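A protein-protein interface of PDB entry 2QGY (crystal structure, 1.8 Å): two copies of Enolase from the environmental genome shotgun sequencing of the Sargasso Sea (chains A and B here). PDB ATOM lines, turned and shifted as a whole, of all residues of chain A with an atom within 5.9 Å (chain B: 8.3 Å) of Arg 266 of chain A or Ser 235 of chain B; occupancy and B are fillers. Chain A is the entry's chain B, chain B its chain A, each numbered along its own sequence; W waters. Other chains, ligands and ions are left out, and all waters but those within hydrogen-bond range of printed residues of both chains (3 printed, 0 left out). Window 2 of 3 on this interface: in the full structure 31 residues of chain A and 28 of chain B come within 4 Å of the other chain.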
ATOM      1  N   ILE A 234     -23.816 -10.690  18.006  1.00  0.00           N
ATOM      2  CA  ILE A 234     -23.352 -11.244  16.739  1.00  0.00           C
ATOM      3  C   ILE A 234     -24.303 -10.875  15.599  1.00  0.00           C
ATOM      4  O   ILE A 234     -23.874 -10.434  14.554  1.00  0.00           O
ATOM      5  CB  ILE A 234     -23.170 -12.753  16.804  1.00  0.00           C
ATOM      6  CG1 ILE A 234     -22.470 -13.204  18.110  1.00  0.00           C
ATOM      7  CG2 ILE A 234     -22.429 -13.235  15.551  1.00  0.00           C
ATOM      8  CD1 ILE A 234     -21.058 -12.732  18.255  1.00  0.00           C
ATOM      9  N   SER A 235     -25.598 -11.013  15.835  1.00  0.00           N
ATOM     10  CA  SER A 235     -26.586 -10.671  14.803  1.00  0.00           C
ATOM     11  C   SER A 235     -26.550  -9.224  14.315  1.00  0.00           C
ATOM     12  O   SER A 235     -26.655  -8.943  13.105  1.00  0.00           O
ATOM     13  CB  SER A 235     -27.962 -11.030  15.347  1.00  0.00           C
ATOM     14  OG  SER A 235     -28.010 -12.444  15.424  1.00  0.00           O
ATOM     15  N   THR A 238     -23.404  -8.658  12.095  1.00  0.00           N
ATOM     16  CA  THR A 238     -23.646  -9.144  10.726  1.00  0.00           C
ATOM     17  C   THR A 238     -24.520  -8.141   9.969  1.00  0.00           C
ATOM     18  O   THR A 238     -24.214  -7.790   8.815  1.00  0.00           O
ATOM     19  CB  THR A 238     -24.286 -10.545  10.725  1.00  0.00           C
ATOM     20  OG1 THR A 238     -23.484 -11.437  11.519  1.00  0.00           O
ATOM     21  CG2 THR A 238     -24.413 -11.110   9.291  1.00  0.00           C
ATOM     22  N   ARG A 261     -14.603 -17.818  16.512  1.00  0.00           N
ATOM     23  CA  ARG A 261     -15.070 -18.776  15.489  1.00  0.00           C
ATOM     24  C   ARG A 261     -16.531 -18.546  15.162  1.00  0.00           C
ATOM     25  O   ARG A 261     -16.940 -18.739  14.024  1.00  0.00           O
ATOM     26  CB  ARG A 261     -14.818 -20.200  15.971  1.00  0.00           C
ATOM     27  CG  ARG A 261     -13.351 -20.558  15.877  1.00  0.00           C
ATOM     28  CD  ARG A 261     -13.030 -21.844  16.595  1.00  0.00           C
ATOM     29  NE  ARG A 261     -11.661 -22.269  16.373  1.00  0.00           N
ATOM     30  CZ  ARG A 261     -11.051 -23.187  17.105  1.00  0.00           C
ATOM     31  NH1 ARG A 261     -11.683 -23.771  18.131  1.00  0.00           N
ATOM     32  NH2 ARG A 261      -9.805 -23.533  16.817  1.00  0.00           N
ATOM     33  N   GLU A 262     -17.317 -18.093  16.142  1.00  0.00           N
ATOM     34  CA  GLU A 262     -18.736 -17.737  15.878  1.00  0.00           C
ATOM     35  C   GLU A 262     -18.816 -16.474  15.007  1.00  0.00           C
ATOM     36  O   GLU A 262     -19.674 -16.368  14.102  1.00  0.00           O
ATOM     37  CB  GLU A 262     -19.517 -17.620  17.184  1.00  0.00           C
ATOM     38  CG  GLU A 262     -20.982 -17.136  17.077  1.00  0.00           C
ATOM     39  CD  GLU A 262     -21.959 -18.063  16.315  1.00  0.00           C
ATOM     40  OE1 GLU A 262     -21.617 -19.198  15.891  1.00  0.00           O
ATOM     41  OE2 GLU A 262     -23.101 -17.610  16.133  1.00  0.00           O
ATOM     42  N   LEU A 263     -17.890 -15.539  15.232  1.00  0.00           N
ATOM     43  CA  LEU A 263     -17.825 -14.320  14.398  1.00  0.00           C
ATOM     44  C   LEU A 263     -17.523 -14.704  12.958  1.00  0.00           C
ATOM     45  O   LEU A 263     -18.091 -14.136  12.028  1.00  0.00           O
ATOM     46  CB  LEU A 263     -16.748 -13.360  14.903  1.00  0.00           C
ATOM     47  CG  LEU A 263     -17.067 -12.649  16.231  1.00  0.00           C
ATOM     48  CD1 LEU A 263     -15.814 -11.850  16.609  1.00  0.00           C
ATOM     49  CD2 LEU A 263     -18.295 -11.747  16.122  1.00  0.00           C
ATOM     50  N   ILE A 264     -16.623 -15.674  12.787  1.00  0.00           N
ATOM     51  CA  ILE A 264     -16.286 -16.157  11.450  1.00  0.00           C
ATOM     52  C   ILE A 264     -17.513 -16.834  10.820  1.00  0.00           C
ATOM     53  O   ILE A 264     -17.904 -16.517   9.687  1.00  0.00           O
ATOM     54  CB  ILE A 264     -15.097 -17.125  11.460  1.00  0.00           C
ATOM     55  CG1 ILE A 264     -13.807 -16.370  11.841  1.00  0.00           C
ATOM     56  CG2 ILE A 264     -15.033 -17.843  10.047  1.00  0.00           C
ATOM     57  CD1 ILE A 264     -12.541 -17.225  12.064  1.00  0.00           C
ATOM     58  N   SER A 265     -18.113 -17.770  11.550  1.00  0.00           N
ATOM     59  CA  SER A 265     -19.295 -18.487  11.057  1.00  0.00           C
ATOM     60  C   SER A 265     -20.396 -17.565  10.586  1.00  0.00           C
ATOM     61  O   SER A 265     -21.105 -17.868   9.609  1.00  0.00           O
ATOM     62  CB  SER A 265     -19.901 -19.350  12.167  1.00  0.00           C
ATOM     63  OG  SER A 265     -19.036 -20.397  12.486  1.00  0.00           O
ATOM     64  N   ARG A 266     -20.618 -16.491  11.341  1.00  0.00           N
ATOM     65  CA  ARG A 266     -21.719 -15.578  11.062  1.00  0.00           C
ATOM     66  C   ARG A 266     -21.363 -14.371  10.180  1.00  0.00           C
ATOM     67  O   ARG A 266     -22.225 -13.511   9.946  1.00  0.00           O
ATOM     68  CB  ARG A 266     -22.348 -15.108  12.365  1.00  0.00           C
ATOM     69  CG  ARG A 266     -22.880 -16.241  13.224  1.00  0.00           C
ATOM     70  CD  ARG A 266     -24.005 -17.025  12.520  1.00  0.00           C
ATOM     71  NE  ARG A 266     -25.262 -16.301  12.365  1.00  0.00           N
ATOM     72  CZ  ARG A 266     -26.403 -16.836  11.906  1.00  0.00           C
ATOM     73  NH1 ARG A 266     -26.465 -18.117  11.533  1.00  0.00           N
ATOM     74  NH2 ARG A 266     -27.498 -16.091  11.842  1.00  0.00           N
ATOM     75  N   ASN A 267     -20.122 -14.334   9.701  1.00  0.00           N
ATOM     76  CA  ASN A 267     -19.643 -13.275   8.818  1.00  0.00           C
ATOM     77  C   ASN A 267     -19.887 -11.920   9.482  1.00  0.00           C
ATOM     78  O   ASN A 267     -20.420 -11.001   8.863  1.00  0.00           O
ATOM     79  CB  ASN A 267     -20.392 -13.380   7.477  1.00  0.00           C
ATOM     80  CG  ASN A 267     -20.090 -14.689   6.781  1.00  0.00           C
ATOM     81  OD1 ASN A 267     -18.922 -14.971   6.450  1.00  0.00           O
ATOM     82  ND2 ASN A 267     -21.108 -15.490   6.562  1.00  0.00           N
ATOM     83  N   ALA A 268     -19.503 -11.832  10.750  1.00  0.00           N
ATOM     84  CA  ALA A 268     -19.865 -10.693  11.605  1.00  0.00           C
ATOM     85  C   ALA A 268     -18.858  -9.547  11.572  1.00  0.00           C
ATOM     86  O   ALA A 268     -19.149  -8.446  12.051  1.00  0.00           O
ATOM     87  CB  ALA A 268     -20.061 -11.192  13.026  1.00  0.00           C
ATOM     88  N   VAL B 229     -23.298 -28.403  23.449  1.00  0.00           N
ATOM     89  CA  VAL B 229     -22.191 -27.732  22.764  1.00  0.00           C
ATOM     90  C   VAL B 229     -21.795 -26.470  23.535  1.00  0.00           C
ATOM     91  O   VAL B 229     -22.527 -26.022  24.398  1.00  0.00           O
ATOM     92  CB  VAL B 229     -22.526 -27.372  21.291  1.00  0.00           C
ATOM     93  CG1 VAL B 229     -22.887 -28.656  20.485  1.00  0.00           C
ATOM     94  CG2 VAL B 229     -23.654 -26.395  21.214  1.00  0.00           C
ATOM     95  N   ASP B 230     -20.665 -25.879  23.169  1.00  0.00           N
ATOM     96  CA  ASP B 230     -20.190 -24.689  23.872  1.00  0.00           C
ATOM     97  C   ASP B 230     -21.226 -23.563  23.773  1.00  0.00           C
ATOM     98  O   ASP B 230     -21.758 -23.302  22.705  1.00  0.00           O
ATOM     99  CB  ASP B 230     -18.847 -24.212  23.300  1.00  0.00           C
ATOM    100  CG  ASP B 230     -18.142 -23.251  24.235  1.00  0.00           C
ATOM    101  OD1 ASP B 230     -18.569 -22.086  24.300  1.00  0.00           O
ATOM    102  OD2 ASP B 230     -17.149 -23.658  24.886  1.00  0.00           O
ATOM    103  N   GLY B 231     -21.485 -22.879  24.891  1.00  0.00           N
ATOM    104  CA  GLY B 231     -22.538 -21.854  24.930  1.00  0.00           C
ATOM    105  C   GLY B 231     -22.250 -20.666  24.027  1.00  0.00           C
ATOM    106  O   GLY B 231     -23.151 -19.924  23.670  1.00  0.00           O
ATOM    107  N   GLU B 232     -20.986 -20.474  23.682  1.00  0.00           N
ATOM    108  CA  GLU B 232     -20.619 -19.395  22.770  1.00  0.00           C
ATOM    109  C   GLU B 232     -20.741 -19.781  21.300  1.00  0.00           C
ATOM    110  O   GLU B 232     -20.714 -18.910  20.428  1.00  0.00           O
ATOM    111  CB  GLU B 232     -19.215 -18.879  23.053  1.00  0.00           C
ATOM    112  CG  GLU B 232     -19.135 -18.104  24.355  1.00  0.00           C
ATOM    113  CD  GLU B 232     -17.797 -17.439  24.514  1.00  0.00           C
ATOM    114  OE1 GLU B 232     -17.591 -16.354  23.937  1.00  0.00           O
ATOM    115  OE2 GLU B 232     -16.954 -18.006  25.224  1.00  0.00           O
ATOM    116  N   ASN B 233     -20.857 -21.078  21.033  1.00  0.00           N
ATOM    117  CA  ASN B 233     -21.023 -21.545  19.651  1.00  0.00           C
ATOM    118  C   ASN B 233     -22.511 -21.576  19.333  1.00  0.00           C
ATOM    119  O   ASN B 233     -23.141 -22.636  19.345  1.00  0.00           O
ATOM    120  CB  ASN B 233     -20.409 -22.939  19.462  1.00  0.00           C
ATOM    121  CG  ASN B 233     -20.269 -23.326  17.967  1.00  0.00           C
ATOM    122  OD1 ASN B 233     -20.963 -22.786  17.104  1.00  0.00           O
ATOM    123  ND2 ASN B 233     -19.343 -24.208  17.678  1.00  0.00           N
ATOM    124  N   ILE B 234     -23.073 -20.400  19.092  1.00  0.00           N
ATOM    125  CA  ILE B 234     -24.514 -20.271  18.942  1.00  0.00           C
ATOM    126  C   ILE B 234     -24.963 -21.038  17.687  1.00  0.00           C
ATOM    127  O   ILE B 234     -26.044 -21.664  17.682  1.00  0.00           O
ATOM    128  CB  ILE B 234     -24.977 -18.776  18.958  1.00  0.00           C
ATOM    129  CG1 ILE B 234     -24.464 -18.086  20.244  1.00  0.00           C
ATOM    130  CG2 ILE B 234     -26.498 -18.669  18.871  1.00  0.00           C
ATOM    131  CD1 ILE B 234     -24.885 -16.633  20.388  1.00  0.00           C
ATOM    132  N   SER B 235     -24.128 -21.000  16.654  1.00  0.00           N
ATOM    133  CA  SER B 235     -24.417 -21.740  15.419  1.00  0.00           C
ATOM    134  C   SER B 235     -24.696 -23.205  15.717  1.00  0.00           C
ATOM    135  O   SER B 235     -25.687 -23.766  15.217  1.00  0.00           O
ATOM    136  CB  SER B 235     -23.251 -21.599  14.436  1.00  0.00           C
ATOM    137  OG  SER B 235     -23.161 -20.248  14.027  1.00  0.00           O
ATOM    138  N   LEU B 236     -23.830 -23.832  16.513  1.00  0.00           N
ATOM    139  CA  LEU B 236     -23.981 -25.251  16.871  1.00  0.00           C
ATOM    140  C   LEU B 236     -25.160 -25.487  17.791  1.00  0.00           C
ATOM    141  O   LEU B 236     -25.853 -26.503  17.678  1.00  0.00           O
ATOM    142  CB  LEU B 236     -22.720 -25.798  17.533  1.00  0.00           C
ATOM    143  CG  LEU B 236     -21.764 -26.604  16.669  1.00  0.00           C
ATOM    144  CD1 LEU B 236     -21.095 -25.709  15.632  1.00  0.00           C
ATOM    145  CD2 LEU B 236     -20.731 -27.314  17.551  1.00  0.00           C
ATOM    146  N   LEU B 237     -25.407 -24.548  18.704  1.00  0.00           N
ATOM    147  CA  LEU B 237     -26.568 -24.696  19.597  1.00  0.00           C
ATOM    148  C   LEU B 237     -27.849 -24.761  18.774  1.00  0.00           C
ATOM    149  O   LEU B 237     -28.738 -25.606  19.011  1.00  0.00           O
ATOM    150  CB  LEU B 237     -26.677 -23.525  20.587  1.00  0.00           C
ATOM    151  CG  LEU B 237     -25.889 -23.515  21.889  1.00  0.00           C
ATOM    152  CD1 LEU B 237     -25.982 -22.096  22.481  1.00  0.00           C
ATOM    153  CD2 LEU B 237     -26.448 -24.543  22.853  1.00  0.00           C
ATOM    154  N   THR B 238     -27.971 -23.843  17.825  1.00  0.00           N
ATOM    155  CA  THR B 238     -29.161 -23.824  16.987  1.00  0.00           C
ATOM    156  C   THR B 238     -29.245 -25.136  16.208  1.00  0.00           C
ATOM    157  O   THR B 238     -30.300 -25.734  16.127  1.00  0.00           O
ATOM    158  CB  THR B 238     -29.221 -22.596  16.064  1.00  0.00           C
ATOM    159  OG1 THR B 238     -28.190 -22.688  15.062  1.00  0.00           O
ATOM    160  CG2 THR B 238     -29.082 -21.276  16.886  1.00  0.00           C
ATOM    161  N   GLU B 239     -28.125 -25.590  15.672  1.00  0.00           N
ATOM    162  CA  GLU B 239     -28.106 -26.838  14.909  1.00  0.00           C
ATOM    163  C   GLU B 239     -28.622 -28.031  15.757  1.00  0.00           C
ATOM    164  O   GLU B 239     -29.463 -28.815  15.303  1.00  0.00           O
ATOM    165  CB  GLU B 239     -26.711 -27.097  14.379  1.00  0.00           C
ATOM    166  CG  GLU B 239     -26.519 -28.501  13.847  1.00  0.00           C
ATOM    167  CD  GLU B 239     -25.199 -28.659  13.158  1.00  0.00           C
ATOM    168  OE1 GLU B 239     -24.649 -27.621  12.712  1.00  0.00           O
ATOM    169  OE2 GLU B 239     -24.735 -29.818  13.044  1.00  0.00           O
ATOM    170  N   ILE B 240     -28.133 -28.145  16.985  1.00  0.00           N
ATOM    171  CA  ILE B 240     -28.598 -29.189  17.914  1.00  0.00           C
ATOM    172  C   ILE B 240     -30.063 -29.070  18.240  1.00  0.00           C
ATOM    173  O   ILE B 240     -30.805 -30.066  18.175  1.00  0.00           O
ATOM    174  CB  ILE B 240     -27.808 -29.193  19.261  1.00  0.00           C
ATOM    175  CG1 ILE B 240     -26.370 -29.679  19.044  1.00  0.00           C
ATOM    176  CG2 ILE B 240     -28.556 -30.054  20.327  1.00  0.00           C
ATOM    177  CD1 ILE B 240     -26.204 -31.174  18.802  1.00  0.00           C
ATOM    178  N   LYS B 241     -30.494 -27.870  18.611  1.00  0.00           N
ATOM    179  CA  LYS B 241     -31.894 -27.666  18.994  1.00  0.00           C
ATOM    180  C   LYS B 241     -32.812 -28.026  17.832  1.00  0.00           C
ATOM    181  O   LYS B 241     -33.899 -28.573  18.050  1.00  0.00           O
ATOM    182  CB  LYS B 241     -32.130 -26.220  19.434  1.00  0.00           C
ATOM    183  CG  LYS B 241     -33.579 -25.858  19.638  1.00  0.00           C
ATOM    184  CD  LYS B 241     -33.725 -24.521  20.330  1.00  0.00           C
ATOM    185  CE  LYS B 241     -35.052 -23.837  19.987  1.00  0.00           C
ATOM    186  NZ  LYS B 241     -36.267 -24.584  20.336  1.00  0.00           N
ATOM    187  N   ASN B 242     -32.354 -27.752  16.614  1.00  0.00           N
ATOM    188  CA  ASN B 242     -33.151 -27.971  15.397  1.00  0.00           C
ATOM    189  C   ASN B 242     -33.192 -29.434  14.959  1.00  0.00           C
ATOM    190  O   ASN B 242     -34.109 -29.841  14.228  1.00  0.00           O
ATOM    191  CB  ASN B 242     -32.626 -27.108  14.233  1.00  0.00           C
ATOM    192  CG  ASN B 242     -32.798 -25.581  14.476  1.00  0.00           C
ATOM    193  OD1 ASN B 242     -33.566 -25.140  15.349  1.00  0.00           O
ATOM    194  ND2 ASN B 242     -32.080 -24.780  13.692  1.00  0.00           N
ATOM    195  N   GLU B 262     -28.676 -12.360  22.330  1.00  0.00           N
ATOM    196  CA  GLU B 262     -28.330 -13.054  21.080  1.00  0.00           C
ATOM    197  C   GLU B 262     -28.938 -14.458  21.058  1.00  0.00           C
ATOM    198  O   GLU B 262     -29.453 -14.871  20.017  1.00  0.00           O
ATOM    199  CB  GLU B 262     -26.816 -13.128  20.890  1.00  0.00           C
ATOM    200  CG  GLU B 262     -26.335 -13.879  19.600  1.00  0.00           C
ATOM    201  CD  GLU B 262     -26.638 -13.141  18.303  1.00  0.00           C
ATOM    202  OE1 GLU B 262     -26.936 -11.939  18.364  1.00  0.00           O
ATOM    203  OE2 GLU B 262     -26.573 -13.777  17.217  1.00  0.00           O
ATOM    204  N   LEU B 263     -28.863 -15.207  22.163  1.00  0.00           N
ATOM    205  CA  LEU B 263     -29.463 -16.564  22.189  1.00  0.00           C
ATOM    206  C   LEU B 263     -30.962 -16.467  21.925  1.00  0.00           C
ATOM    207  O   LEU B 263     -31.514 -17.263  21.182  1.00  0.00           O
ATOM    208  CB  LEU B 263     -29.242 -17.287  23.532  1.00  0.00           C
ATOM    209  CG  LEU B 263     -27.806 -17.638  23.938  1.00  0.00           C
ATOM    210  CD1 LEU B 263     -27.892 -18.094  25.388  1.00  0.00           C
ATOM    211  CD2 LEU B 263     -27.279 -18.796  23.067  1.00  0.00           C
ATOM    212  N   SER B 265     -32.520 -14.126  20.189  1.00  0.00           N
ATOM    213  CA  SER B 265     -32.638 -13.672  18.785  1.00  0.00           C
ATOM    214  C   SER B 265     -32.531 -14.826  17.835  1.00  0.00           C
ATOM    215  O   SER B 265     -33.194 -14.865  16.794  1.00  0.00           O
ATOM    216  CB  SER B 265     -31.490 -12.718  18.427  1.00  0.00           C
ATOM    217  OG  SER B 265     -31.667 -11.455  19.017  1.00  0.00           O
ATOM    218  N   ARG B 266     -31.649 -15.753  18.194  1.00  0.00           N
ATOM    219  CA  ARG B 266     -31.293 -16.865  17.344  1.00  0.00           C
ATOM    220  C   ARG B 266     -32.110 -18.141  17.604  1.00  0.00           C
ATOM    221  O   ARG B 266     -31.830 -19.178  16.999  1.00  0.00           O
ATOM    222  CB  ARG B 266     -29.799 -17.171  17.525  1.00  0.00           C
ATOM    223  CG  ARG B 266     -28.835 -16.031  17.069  1.00  0.00           C
ATOM    224  CD  ARG B 266     -28.478 -16.116  15.581  1.00  0.00           C
ATOM    225  NE  ARG B 266     -27.632 -17.269  15.316  1.00  0.00           N
ATOM    226  CZ  ARG B 266     -26.311 -17.322  15.567  1.00  0.00           C
ATOM    227  NH1 ARG B 266     -25.643 -18.430  15.292  1.00  0.00           N
ATOM    228  NH2 ARG B 266     -25.646 -16.277  16.070  1.00  0.00           N
ATOM    229  N   ALA B 268     -31.885 -20.126  20.103  1.00  0.00           N
ATOM    230  CA  ALA B 268     -30.801 -21.080  20.251  1.00  0.00           C
ATOM    231  C   ALA B 268     -30.959 -22.058  21.423  1.00  0.00           C
ATOM    232  O   ALA B 268     -30.178 -23.006  21.558  1.00  0.00           O
ATOM    233  CB  ALA B 268     -29.443 -20.344  20.332  1.00  0.00           C
HETATM  234  O   HOH W   1     -23.983 -20.160  11.292  1.00  0.00           O
HETATM  235  O   HOH W   2     -17.924 -21.090  17.698  1.00  0.00           O
HETATM  236  O   HOH W   3     -19.658 -21.040  15.500  1.00  0.00           O
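Ser 235 of chain A touches Arg 266 of chain B, and with the chains exchanged Arg 266 of chain A touches Ser 235 of chain B.
Glu 262 of chain A touches Arg 266 of chain B, but with the chains exchanged Arg 266 of chain A does not touch Glu 262 of chain B (5.6 Å).
Ser 265 of chain A touches Ser 235 of chain B, but with the chains exchanged Ser 235 of chain A does not touch Ser 265 of chain B (4.6 Å).
Arg 266 of chain A touches its own counterpart, Arg 266 of chain B.
8 positions are printed for both chains.
The guanidinium group of Arg 266 of chain B lies within hydrogen-bond range of the side-chain hydroxyl of Ser 235 of chain B (3.3 Å).
O of Ser 235 of chain B lies within hydrogen-bond range of OG1 of Thr 238 of chain B, 2.7 Å away.
The backbone NH of Leu 236 of chain B sits at hydrogen-bond distance from the side-chain amide oxygen of Asn 233 of chain B.
The backbone carbonyl oxygen (O) of Ile 234 of chain A lies within hydrogen-bond range of the side-chain hydroxyl (OG1) of Thr 238 of chain A (3.2 Å).
The side-chain carboxylate of Asp 230 of chain B sits at hydrogen-bond distance from the backbone NH of Glu 232 of chain B (3.0 Å).
The side-chain hydroxyl (OG1) of Thr 238 of chain A sits at hydrogen-bond distance from the backbone carbonyl oxygen (O) of Arg 266 of chain A.
Of the 19 printed residues of chain B, 6 touch a printed residue of chain A.
Among the printed residues, 11 pairs touch across the chains.
Water W3 lies within hydrogen-bond range of OD1 of Asn 233 of chain B (2.7 Å), OE1 of Glu 262 of chain A (2.7 Å) and OG of Ser 265 of chain A (3.1 Å).
Water W1 bridges OG of Ser 235 of chain B (2.9 Å) and NH1 of Arg 266 of chain A (3.2 Å).
Water W2 lies within hydrogen-bond range of ND2 of Asn 233 of chain B (3.4 Å) and N of Glu 262 of chain A (3.4 Å).
Of chain B, only Ser 235 (3.7 Å) and Arg 266 (3.5 Å) come within 4 Å of Arg 266 of chain A.
Ser 235 of chain B touches three residues of chain A.
Of the printed residues of chain B, Ser 235 of chain A touches Glu 262 (2.7 Å) and Arg 266 (3.7 Å).
Of the printed residues of chain A, Asn 233 of chain B touches Glu 262.
Of the printed residues of chain B, Ser 265 of chain A touches Ser 235 (3.9 Å).
Printed residues of chain A within 4 Å of Ile 234 of chain B: Glu 262.
Of the printed residues of chain B, Ile 234 of chain A touches Glu 262.
Leu 236 of chain B touches none of the printed residues of chain A.
Thr 238 of chain B touches none of the printed residues of chain A.
The nearest residue of chain B that does not touch Arg 266 of chain A is Glu 262 of chain B (5.6 Å).
OE1 of Glu 262 of chain B is in hydrogen-bond range of N of Ile 234 of chain A, at 3.4 Å.
OG of Ser 235 of chain A is in hydrogen-bond range of OE2 of Glu 262 of chain B (2.7 Å).
The guanidinium group of Arg 266 of chain B lies within salt-bridge range of the side-chain carboxylate of Glu 262 of chain A.
The side-chain hydroxyl of Ser 235 of chain B sits at hydrogen-bond distance from the side-chain carboxylate of Glu 262 of chain A.
Among the printed residues, pairs that only touch across the chains: Arg 266 of chain A with Arg 266 of chain B (3.5 Å), Glu 262 of chain A with Ile 234 of chain B (3.6 Å), Arg 266 of chain A with Ser 235 of chain B (3.7 Å), Glu 262 of chain A with Glu 232 of chain B (3.7 Å), Ser 235 of chain A with Arg 266 of chain B (3.7 Å), Glu 262 of chain A with Asn 233 of chain B (3.8 Å) and Ser 265 of chain A with Ser 235 of chain B (3.9 Å).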
